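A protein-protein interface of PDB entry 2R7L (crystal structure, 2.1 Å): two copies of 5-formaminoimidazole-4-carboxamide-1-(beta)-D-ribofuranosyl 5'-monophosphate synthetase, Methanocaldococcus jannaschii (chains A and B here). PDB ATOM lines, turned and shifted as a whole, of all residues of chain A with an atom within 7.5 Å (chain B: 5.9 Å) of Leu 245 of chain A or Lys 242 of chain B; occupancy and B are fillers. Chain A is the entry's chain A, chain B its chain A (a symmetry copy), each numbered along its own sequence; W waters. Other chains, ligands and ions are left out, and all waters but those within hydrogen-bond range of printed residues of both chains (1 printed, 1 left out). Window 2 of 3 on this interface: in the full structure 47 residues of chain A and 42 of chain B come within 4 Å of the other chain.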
ATOM      1  N   SER A 170      25.861 -13.264 -19.790  1.00  0.00           N
ATOM      2  CA  SER A 170      26.776 -12.124 -19.771  1.00  0.00           C
ATOM      3  C   SER A 170      26.057 -10.768 -19.794  1.00  0.00           C
ATOM      4  O   SER A 170      26.704  -9.719 -19.825  1.00  0.00           O
ATOM      5  CB  SER A 170      27.803 -12.219 -20.903  1.00  0.00           C
ATOM      6  OG  SER A 170      28.806 -13.184 -20.607  1.00  0.00           O
ATOM      7  N   GLU A 174      20.508 -11.496 -21.893  1.00  0.00           N
ATOM      8  CA  GLU A 174      20.815 -12.912 -22.056  1.00  0.00           C
ATOM      9  C   GLU A 174      20.174 -13.761 -20.961  1.00  0.00           C
ATOM     10  O   GLU A 174      19.670 -14.854 -21.224  1.00  0.00           O
ATOM     11  CB  GLU A 174      22.320 -13.143 -22.088  1.00  0.00           C
ATOM     12  CG  GLU A 174      22.687 -14.606 -22.111  1.00  0.00           C
ATOM     13  CD  GLU A 174      24.069 -14.851 -22.665  1.00  0.00           C
ATOM     14  OE1 GLU A 174      25.007 -14.105 -22.301  1.00  0.00           O
ATOM     15  OE2 GLU A 174      24.211 -15.801 -23.465  1.00  0.00           O
ATOM     16  N   LYS A 178      17.732 -16.920 -21.972  1.00  0.00           N
ATOM     17  CA  LYS A 178      18.018 -18.285 -21.532  1.00  0.00           C
ATOM     18  C   LYS A 178      16.991 -18.849 -20.557  1.00  0.00           C
ATOM     19  O   LYS A 178      16.589 -20.008 -20.673  1.00  0.00           O
ATOM     20  CB  LYS A 178      19.427 -18.385 -20.947  1.00  0.00           C
ATOM     21  CG  LYS A 178      20.467 -18.684 -22.003  1.00  0.00           C
ATOM     22  CD  LYS A 178      21.866 -18.426 -21.510  1.00  0.00           C
ATOM     23  CE  LYS A 178      22.863 -18.762 -22.598  1.00  0.00           C
ATOM     24  NZ  LYS A 178      24.250 -18.759 -22.079  1.00  0.00           N
ATOM     25  N   ILE A 239      33.585 -30.746 -27.608  1.00  0.00           N
ATOM     26  CA  ILE A 239      33.167 -30.586 -29.007  1.00  0.00           C
ATOM     27  C   ILE A 239      33.847 -29.321 -29.520  1.00  0.00           C
ATOM     28  O   ILE A 239      33.813 -28.290 -28.847  1.00  0.00           O
ATOM     29  CB  ILE A 239      31.640 -30.428 -29.110  1.00  0.00           C
ATOM     30  CG1 ILE A 239      30.939 -31.636 -28.488  1.00  0.00           C
ATOM     31  CG2 ILE A 239      31.185 -30.265 -30.569  1.00  0.00           C
ATOM     32  CD1 ILE A 239      29.439 -31.453 -28.331  1.00  0.00           C
ATOM     33  N   PRO A 240      34.497 -29.399 -30.696  1.00  0.00           N
ATOM     34  CA  PRO A 240      35.154 -28.221 -31.284  1.00  0.00           C
ATOM     35  C   PRO A 240      34.175 -27.056 -31.453  1.00  0.00           C
ATOM     36  O   PRO A 240      32.987 -27.277 -31.689  1.00  0.00           O
ATOM     37  CB  PRO A 240      35.634 -28.730 -32.648  1.00  0.00           C
ATOM     38  CG  PRO A 240      35.760 -30.212 -32.470  1.00  0.00           C
ATOM     39  CD  PRO A 240      34.648 -30.595 -31.542  1.00  0.00           C
ATOM     40  N   ALA A 241      34.673 -25.836 -31.292  1.00  0.00           N
ATOM     41  CA  ALA A 241      33.836 -24.634 -31.297  1.00  0.00           C
ATOM     42  C   ALA A 241      32.921 -24.545 -32.525  1.00  0.00           C
ATOM     43  O   ALA A 241      31.730 -24.228 -32.407  1.00  0.00           O
ATOM     44  CB  ALA A 241      34.712 -23.392 -31.196  1.00  0.00           C
ATOM     45  N   LYS A 242      33.477 -24.835 -33.696  1.00  0.00           N
ATOM     46  CA  LYS A 242      32.716 -24.746 -34.943  1.00  0.00           C
ATOM     47  C   LYS A 242      31.504 -25.656 -34.906  1.00  0.00           C
ATOM     48  O   LYS A 242      30.432 -25.301 -35.389  1.00  0.00           O
ATOM     49  CB  LYS A 242      33.601 -25.087 -36.145  1.00  0.00           C
ATOM     50  CG  LYS A 242      34.601 -23.988 -36.499  1.00  0.00           C
ATOM     51  CD  LYS A 242      35.673 -24.493 -37.451  1.00  0.00           C
ATOM     52  CE  LYS A 242      36.778 -23.461 -37.661  1.00  0.00           C
ATOM     53  NZ  LYS A 242      36.344 -22.336 -38.533  1.00  0.00           N
ATOM     54  N   ASP A 243      31.665 -26.832 -34.316  1.00  0.00           N
ATOM     55  CA  ASP A 243      30.544 -27.756 -34.183  1.00  0.00           C
ATOM     56  C   ASP A 243      29.582 -27.380 -33.053  1.00  0.00           C
ATOM     57  O   ASP A 243      28.379 -27.587 -33.173  1.00  0.00           O
ATOM     58  CB  ASP A 243      31.064 -29.178 -34.037  1.00  0.00           C
ATOM     59  CG  ASP A 243      31.878 -29.601 -35.230  1.00  0.00           C
ATOM     60  OD1 ASP A 243      31.296 -29.661 -36.335  1.00  0.00           O
ATOM     61  OD2 ASP A 243      33.093 -29.852 -35.076  1.00  0.00           O
ATOM     62  N   GLN A 244      30.103 -26.822 -31.960  1.00  0.00           N
ATOM     63  CA  GLN A 244      29.230 -26.366 -30.878  1.00  0.00           C
ATOM     64  C   GLN A 244      28.243 -25.318 -31.387  1.00  0.00           C
ATOM     65  O   GLN A 244      27.057 -25.367 -31.070  1.00  0.00           O
ATOM     66  CB  GLN A 244      30.039 -25.775 -29.722  1.00  0.00           C
ATOM     67  CG  GLN A 244      30.636 -26.792 -28.765  1.00  0.00           C
ATOM     68  CD  GLN A 244      31.302 -26.124 -27.590  1.00  0.00           C
ATOM     69  OE1 GLN A 244      30.678 -25.338 -26.870  1.00  0.00           O
ATOM     70  NE2 GLN A 244      32.582 -26.414 -27.393  1.00  0.00           N
ATOM     71  N   LEU A 245      28.745 -24.367 -32.173  1.00  0.00           N
ATOM     72  CA  LEU A 245      27.917 -23.299 -32.736  1.00  0.00           C
ATOM     73  C   LEU A 245      26.792 -23.818 -33.627  1.00  0.00           C
ATOM     74  O   LEU A 245      25.760 -23.168 -33.770  1.00  0.00           O
ATOM     75  CB  LEU A 245      28.772 -22.297 -33.514  1.00  0.00           C
ATOM     76  CG  LEU A 245      29.883 -21.612 -32.718  1.00  0.00           C
ATOM     77  CD1 LEU A 245      30.538 -20.540 -33.564  1.00  0.00           C
ATOM     78  CD2 LEU A 245      29.354 -21.034 -31.410  1.00  0.00           C
ATOM     79  N   GLU A 246      26.995 -24.987 -34.225  1.00  0.00           N
ATOM     80  CA  GLU A 246      25.977 -25.597 -35.072  1.00  0.00           C
ATOM     81  C   GLU A 246      24.958 -26.406 -34.288  1.00  0.00           C
ATOM     82  O   GLU A 246      24.020 -26.949 -34.868  1.00  0.00           O
ATOM     83  CB  GLU A 246      26.626 -26.503 -36.110  1.00  0.00           C
ATOM     84  CG  GLU A 246      27.341 -25.758 -37.209  1.00  0.00           C
ATOM     85  CD  GLU A 246      28.101 -26.691 -38.117  1.00  0.00           C
ATOM     86  OE1 GLU A 246      28.945 -27.462 -37.606  1.00  0.00           O
ATOM     87  OE2 GLU A 246      27.857 -26.656 -39.341  1.00  0.00           O
ATOM     88  N   MET A 247      25.144 -26.504 -32.976  1.00  0.00           N
ATOM     89  CA  MET A 247      24.258 -27.320 -32.148  1.00  0.00           C
ATOM     90  C   MET A 247      23.344 -26.452 -31.298  1.00  0.00           C
ATOM     91  O   MET A 247      23.691 -25.321 -30.946  1.00  0.00           O
ATOM     92  CB  MET A 247      25.068 -28.242 -31.232  1.00  0.00           C
ATOM     93  CG  MET A 247      26.077 -29.123 -31.946  1.00  0.00           C
ATOM     94  SD  MET A 247      27.212 -29.920 -30.788  1.00  0.00           S
ATOM     95  CE  MET A 247      26.099 -31.040 -29.933  1.00  0.00           C
ATOM     96  N   ASN A 248      22.175 -26.987 -30.968  1.00  0.00           N
ATOM     97  CA  ASN A 248      21.283 -26.324 -30.027  1.00  0.00           C
ATOM     98  C   ASN A 248      21.308 -27.080 -28.708  1.00  0.00           C
ATOM     99  O   ASN A 248      20.421 -27.886 -28.416  1.00  0.00           O
ATOM    100  CB  ASN A 248      19.862 -26.234 -30.590  1.00  0.00           C
ATOM    101  CG  ASN A 248      19.788 -25.393 -31.856  1.00  0.00           C
ATOM    102  OD1 ASN A 248      20.412 -24.331 -31.950  1.00  0.00           O
ATOM    103  ND2 ASN A 248      19.024 -25.865 -32.837  1.00  0.00           N
ATOM    104  N   ILE A 249      22.341 -26.818 -27.914  1.00  0.00           N
ATOM    105  CA  ILE A 249      22.599 -27.601 -26.718  1.00  0.00           C
ATOM    106  C   ILE A 249      22.928 -26.691 -25.543  1.00  0.00           C
ATOM    107  O   ILE A 249      23.725 -25.762 -25.668  1.00  0.00           O
ATOM    108  CB  ILE A 249      23.751 -28.610 -26.967  1.00  0.00           C
ATOM    109  CG1 ILE A 249      23.950 -29.542 -25.767  1.00  0.00           C
ATOM    110  CG2 ILE A 249      25.040 -27.876 -27.329  1.00  0.00           C
ATOM    111  CD1 ILE A 249      24.903 -30.696 -26.053  1.00  0.00           C
ATOM    112  N   ASN A 250      22.293 -26.948 -24.406  1.00  0.00           N
ATOM    113  CA  ASN A 250      22.588 -26.202 -23.192  1.00  0.00           C
ATOM    114  C   ASN A 250      23.481 -27.025 -22.274  1.00  0.00           C
ATOM    115  O   ASN A 250      23.337 -28.248 -22.199  1.00  0.00           O
ATOM    116  CB  ASN A 250      21.295 -25.842 -22.461  1.00  0.00           C
ATOM    117  CG  ASN A 250      20.357 -25.011 -23.312  1.00  0.00           C
ATOM    118  OD1 ASN A 250      19.239 -25.434 -23.616  1.00  0.00           O
ATOM    119  ND2 ASN A 250      20.810 -23.827 -23.712  1.00  0.00           N
ATOM    120  N   PRO B 240      31.336 -22.976 -22.576  1.00  0.00           N
ATOM    121  CA  PRO B 240      30.830 -23.315 -23.915  1.00  0.00           C
ATOM    122  C   PRO B 240      31.139 -22.211 -24.930  1.00  0.00           C
ATOM    123  O   PRO B 240      31.180 -21.034 -24.569  1.00  0.00           O
ATOM    124  CB  PRO B 240      29.319 -23.446 -23.698  1.00  0.00           C
ATOM    125  CG  PRO B 240      29.176 -23.772 -22.242  1.00  0.00           C
ATOM    126  CD  PRO B 240      30.271 -23.010 -21.560  1.00  0.00           C
ATOM    127  N   ALA B 241      31.393 -22.603 -26.173  1.00  0.00           N
ATOM    128  CA  ALA B 241      31.828 -21.676 -27.221  1.00  0.00           C
ATOM    129  C   ALA B 241      30.916 -20.451 -27.354  1.00  0.00           C
ATOM    130  O   ALA B 241      31.393 -19.313 -27.464  1.00  0.00           O
ATOM    131  CB  ALA B 241      31.931 -22.409 -28.551  1.00  0.00           C
ATOM    132  N   LYS B 242      29.608 -20.685 -27.333  1.00  0.00           N
ATOM    133  CA  LYS B 242      28.638 -19.600 -27.493  1.00  0.00           C
ATOM    134  C   LYS B 242      28.814 -18.549 -26.414  1.00  0.00           C
ATOM    135  O   LYS B 242      28.698 -17.354 -26.671  1.00  0.00           O
ATOM    136  CB  LYS B 242      27.207 -20.144 -27.476  1.00  0.00           C
ATOM    137  CG  LYS B 242      26.821 -20.884 -28.756  1.00  0.00           C
ATOM    138  CD  LYS B 242      25.547 -21.694 -28.571  1.00  0.00           C
ATOM    139  CE  LYS B 242      25.257 -22.581 -29.779  1.00  0.00           C
ATOM    140  NZ  LYS B 242      24.753 -21.805 -30.944  1.00  0.00           N
ATOM    141  N   ASP B 243      29.112 -18.992 -25.201  1.00  0.00           N
ATOM    142  CA  ASP B 243      29.353 -18.057 -24.108  1.00  0.00           C
ATOM    143  C   ASP B 243      30.742 -17.415 -24.157  1.00  0.00           C
ATOM    144  O   ASP B 243      30.899 -16.255 -23.790  1.00  0.00           O
ATOM    145  CB  ASP B 243      29.092 -18.743 -22.776  1.00  0.00           C
ATOM    146  CG  ASP B 243      27.671 -19.231 -22.667  1.00  0.00           C
ATOM    147  OD1 ASP B 243      26.762 -18.373 -22.688  1.00  0.00           O
ATOM    148  OD2 ASP B 243      27.459 -20.460 -22.584  1.00  0.00           O
ATOM    149  N   GLN B 244      31.749 -18.158 -24.615  1.00  0.00           N
ATOM    150  CA  GLN B 244      33.085 -17.579 -24.763  1.00  0.00           C
ATOM    151  C   GLN B 244      33.052 -16.385 -25.714  1.00  0.00           C
ATOM    152  O   GLN B 244      33.649 -15.347 -25.438  1.00  0.00           O
ATOM    153  CB  GLN B 244      34.084 -18.613 -25.289  1.00  0.00           C
ATOM    154  CG  GLN B 244      34.647 -19.557 -24.241  1.00  0.00           C
ATOM    155  CD  GLN B 244      35.714 -20.451 -24.817  1.00  0.00           C
ATOM    156  OE1 GLN B 244      36.705 -19.973 -25.380  1.00  0.00           O
ATOM    157  NE2 GLN B 244      35.518 -21.758 -24.699  1.00  0.00           N
ATOM    158  N   LEU B 245      32.355 -16.544 -26.838  1.00  0.00           N
ATOM    159  CA  LEU B 245      32.236 -15.483 -27.841  1.00  0.00           C
ATOM    160  C   LEU B 245      31.582 -14.217 -27.298  1.00  0.00           C
ATOM    161  O   LEU B 245      31.833 -13.123 -27.797  1.00  0.00           O
ATOM    162  CB  LEU B 245      31.466 -15.978 -29.068  1.00  0.00           C
ATOM    163  CG  LEU B 245      32.062 -17.189 -29.785  1.00  0.00           C
ATOM    164  CD1 LEU B 245      31.294 -17.464 -31.060  1.00  0.00           C
ATOM    165  CD2 LEU B 245      33.547 -16.988 -30.071  1.00  0.00           C
ATOM    166  N   GLU B 246      30.744 -14.366 -26.278  1.00  0.00           N
ATOM    167  CA  GLU B 246      30.088 -13.222 -25.657  1.00  0.00           C
ATOM    168  C   GLU B 246      30.942 -12.553 -24.591  1.00  0.00           C
ATOM    169  O   GLU B 246      30.532 -11.554 -24.007  1.00  0.00           O
ATOM    170  CB  GLU B 246      28.769 -13.647 -25.028  1.00  0.00           C
ATOM    171  CG  GLU B 246      27.682 -13.944 -26.031  1.00  0.00           C
ATOM    172  CD  GLU B 246      26.450 -14.513 -25.373  1.00  0.00           C
ATOM    173  OE1 GLU B 246      26.574 -15.542 -24.671  1.00  0.00           O
ATOM    174  OE2 GLU B 246      25.360 -13.935 -25.555  1.00  0.00           O
HETATM  175  O   HOH W   1      28.175 -23.590 -27.213  1.00  0.00           O
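Among the printed residues, merely in contact across the chains: Met 247 of chain A with Lys 242 of chain B (3.4 Å), Gln 244 of chain A with Lys 242 of chain B (3.6 Å), Gln 244 of chain A with Pro 240 of chain B (3.6 Å), Glu 174 of chain A with Asp 243 of chain B (3.7 Å) and Ala 241 of chain A with Ala 241 of chain B (3.96 Å).
Printed residues of chain B within 4 Å of Glu 174 of chain A: Asp 243 (3.7 Å) and Glu 246 (2.7 Å). Of the printed residues of chain B, Lys 178 of chain A touches Asp 243. Printed residues of chain B within 4 Å of Ala 241 of chain A: Ala 241 (3.96 Å). Lys 242 of chain A touches none of the printed residues of chain B. Leu 245 of chain A touches just one residue of chain B: Lys 242 (3.3 Å). Of the printed residues of chain A, Pro 240 of chain B touches Gln 244 (3.6 Å). Of chain A, only Ala 241 (3.96 Å) and Gln 244 (2.9 Å) come within 4 Å of Ala 241 of chain B. Lys 242 of chain B touches just these residues of chain A: Gln 244, Leu 245 and Met 247. Of the printed residues of chain A, Asp 243 of chain B touches Glu 174 and Lys 178. The nearest residue of chain A that does not touch Lys 242 of chain B is Glu 246 of chain A (5.1 Å). The nearest printed residue of chain B that does not touch Gln 244 of chain A is Gln 244 of chain B (6.1 Å).
Of the 7 printed residues of chain B, 5 touch a printed residue of chain A. Printed residues of chain A that touch a printed residue of chain B: Glu 174, Lys 178, Ala 241, Gln 244, Leu 245 and Met 247. Hydrophobic or aromatic side chains of chain A that line the printed part of chain B: Ala 241 and Leu 245. Among the printed residues, 9 pairs touch across the chains. Among the printed residues, Asp or Glu carboxylates within 4 Å of a Lys or Arg side-chain nitrogen of the other chain: Lys 178 of chain A with Asp 243 of chain B (2.6 Å).
The backbone NH (N) of Ser 170 of chain A sits at hydrogen-bond distance from the side-chain carboxylate (OE1) of Glu 174 of chain A (2.8 Å). OE2 of Glu 174 of chain A lies within salt-bridge range of NZ of Lys 178 of chain A (3.3 Å). The backbone carbonyl oxygen (O) of Ile 239 of chain A is in hydrogen-bond range of the side-chain amide nitrogen (NE2) of Gln 244 of chain A (2.7 Å).
Water W1 bridges the side-chain amide oxygen of Gln 244 of chain A and the backbone NH of Lys 242 of chain B.
The side-chain carboxylate (OE1) of Glu 246 of chain B lies close to the side-chain carboxylate (OE2) of Glu 174 of chain A (2.7 Å). OD1 of Asp 243 of chain B lies within salt-bridge range of NZ of Lys 178 of chain A (2.6 Å). The side-chain amide oxygen (OE1) of Gln 244 of chain A sits at hydrogen-bond distance from the backbone NH (N) of Ala 241 of chain B (2.9 Å). O of Leu 245 of chain A sits at hydrogen-bond distance from NZ of Lys 242 of chain B, at 3.3 Å.
Ala 241 of chain B touches its own counterpart, Ala 241 of chain A. Gln 244 of chain A touches Pro 240 of chain B, but with the chains exchanged Pro 240 of chain A does not touch Gln 244 of chain B (8.7 Å). Gln 244 of chain A touches Ala 241 of chain B, but with the chains exchanged Ala 241 of chain A does not touch Gln 244 of chain B (6.7 Å). Leu 245 of chain A touches Lys 242 of chain B, but with the chains exchanged Lys 242 of chain A does not touch Leu 245 of chain B (8.1 Å). Positions printed for both chains: 240, 241, 242, 243, 244, 245 and 246. Of the 9 pairs that touch across the chains among the printed residues, 1 has its exchanged pair printed and touching as well.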
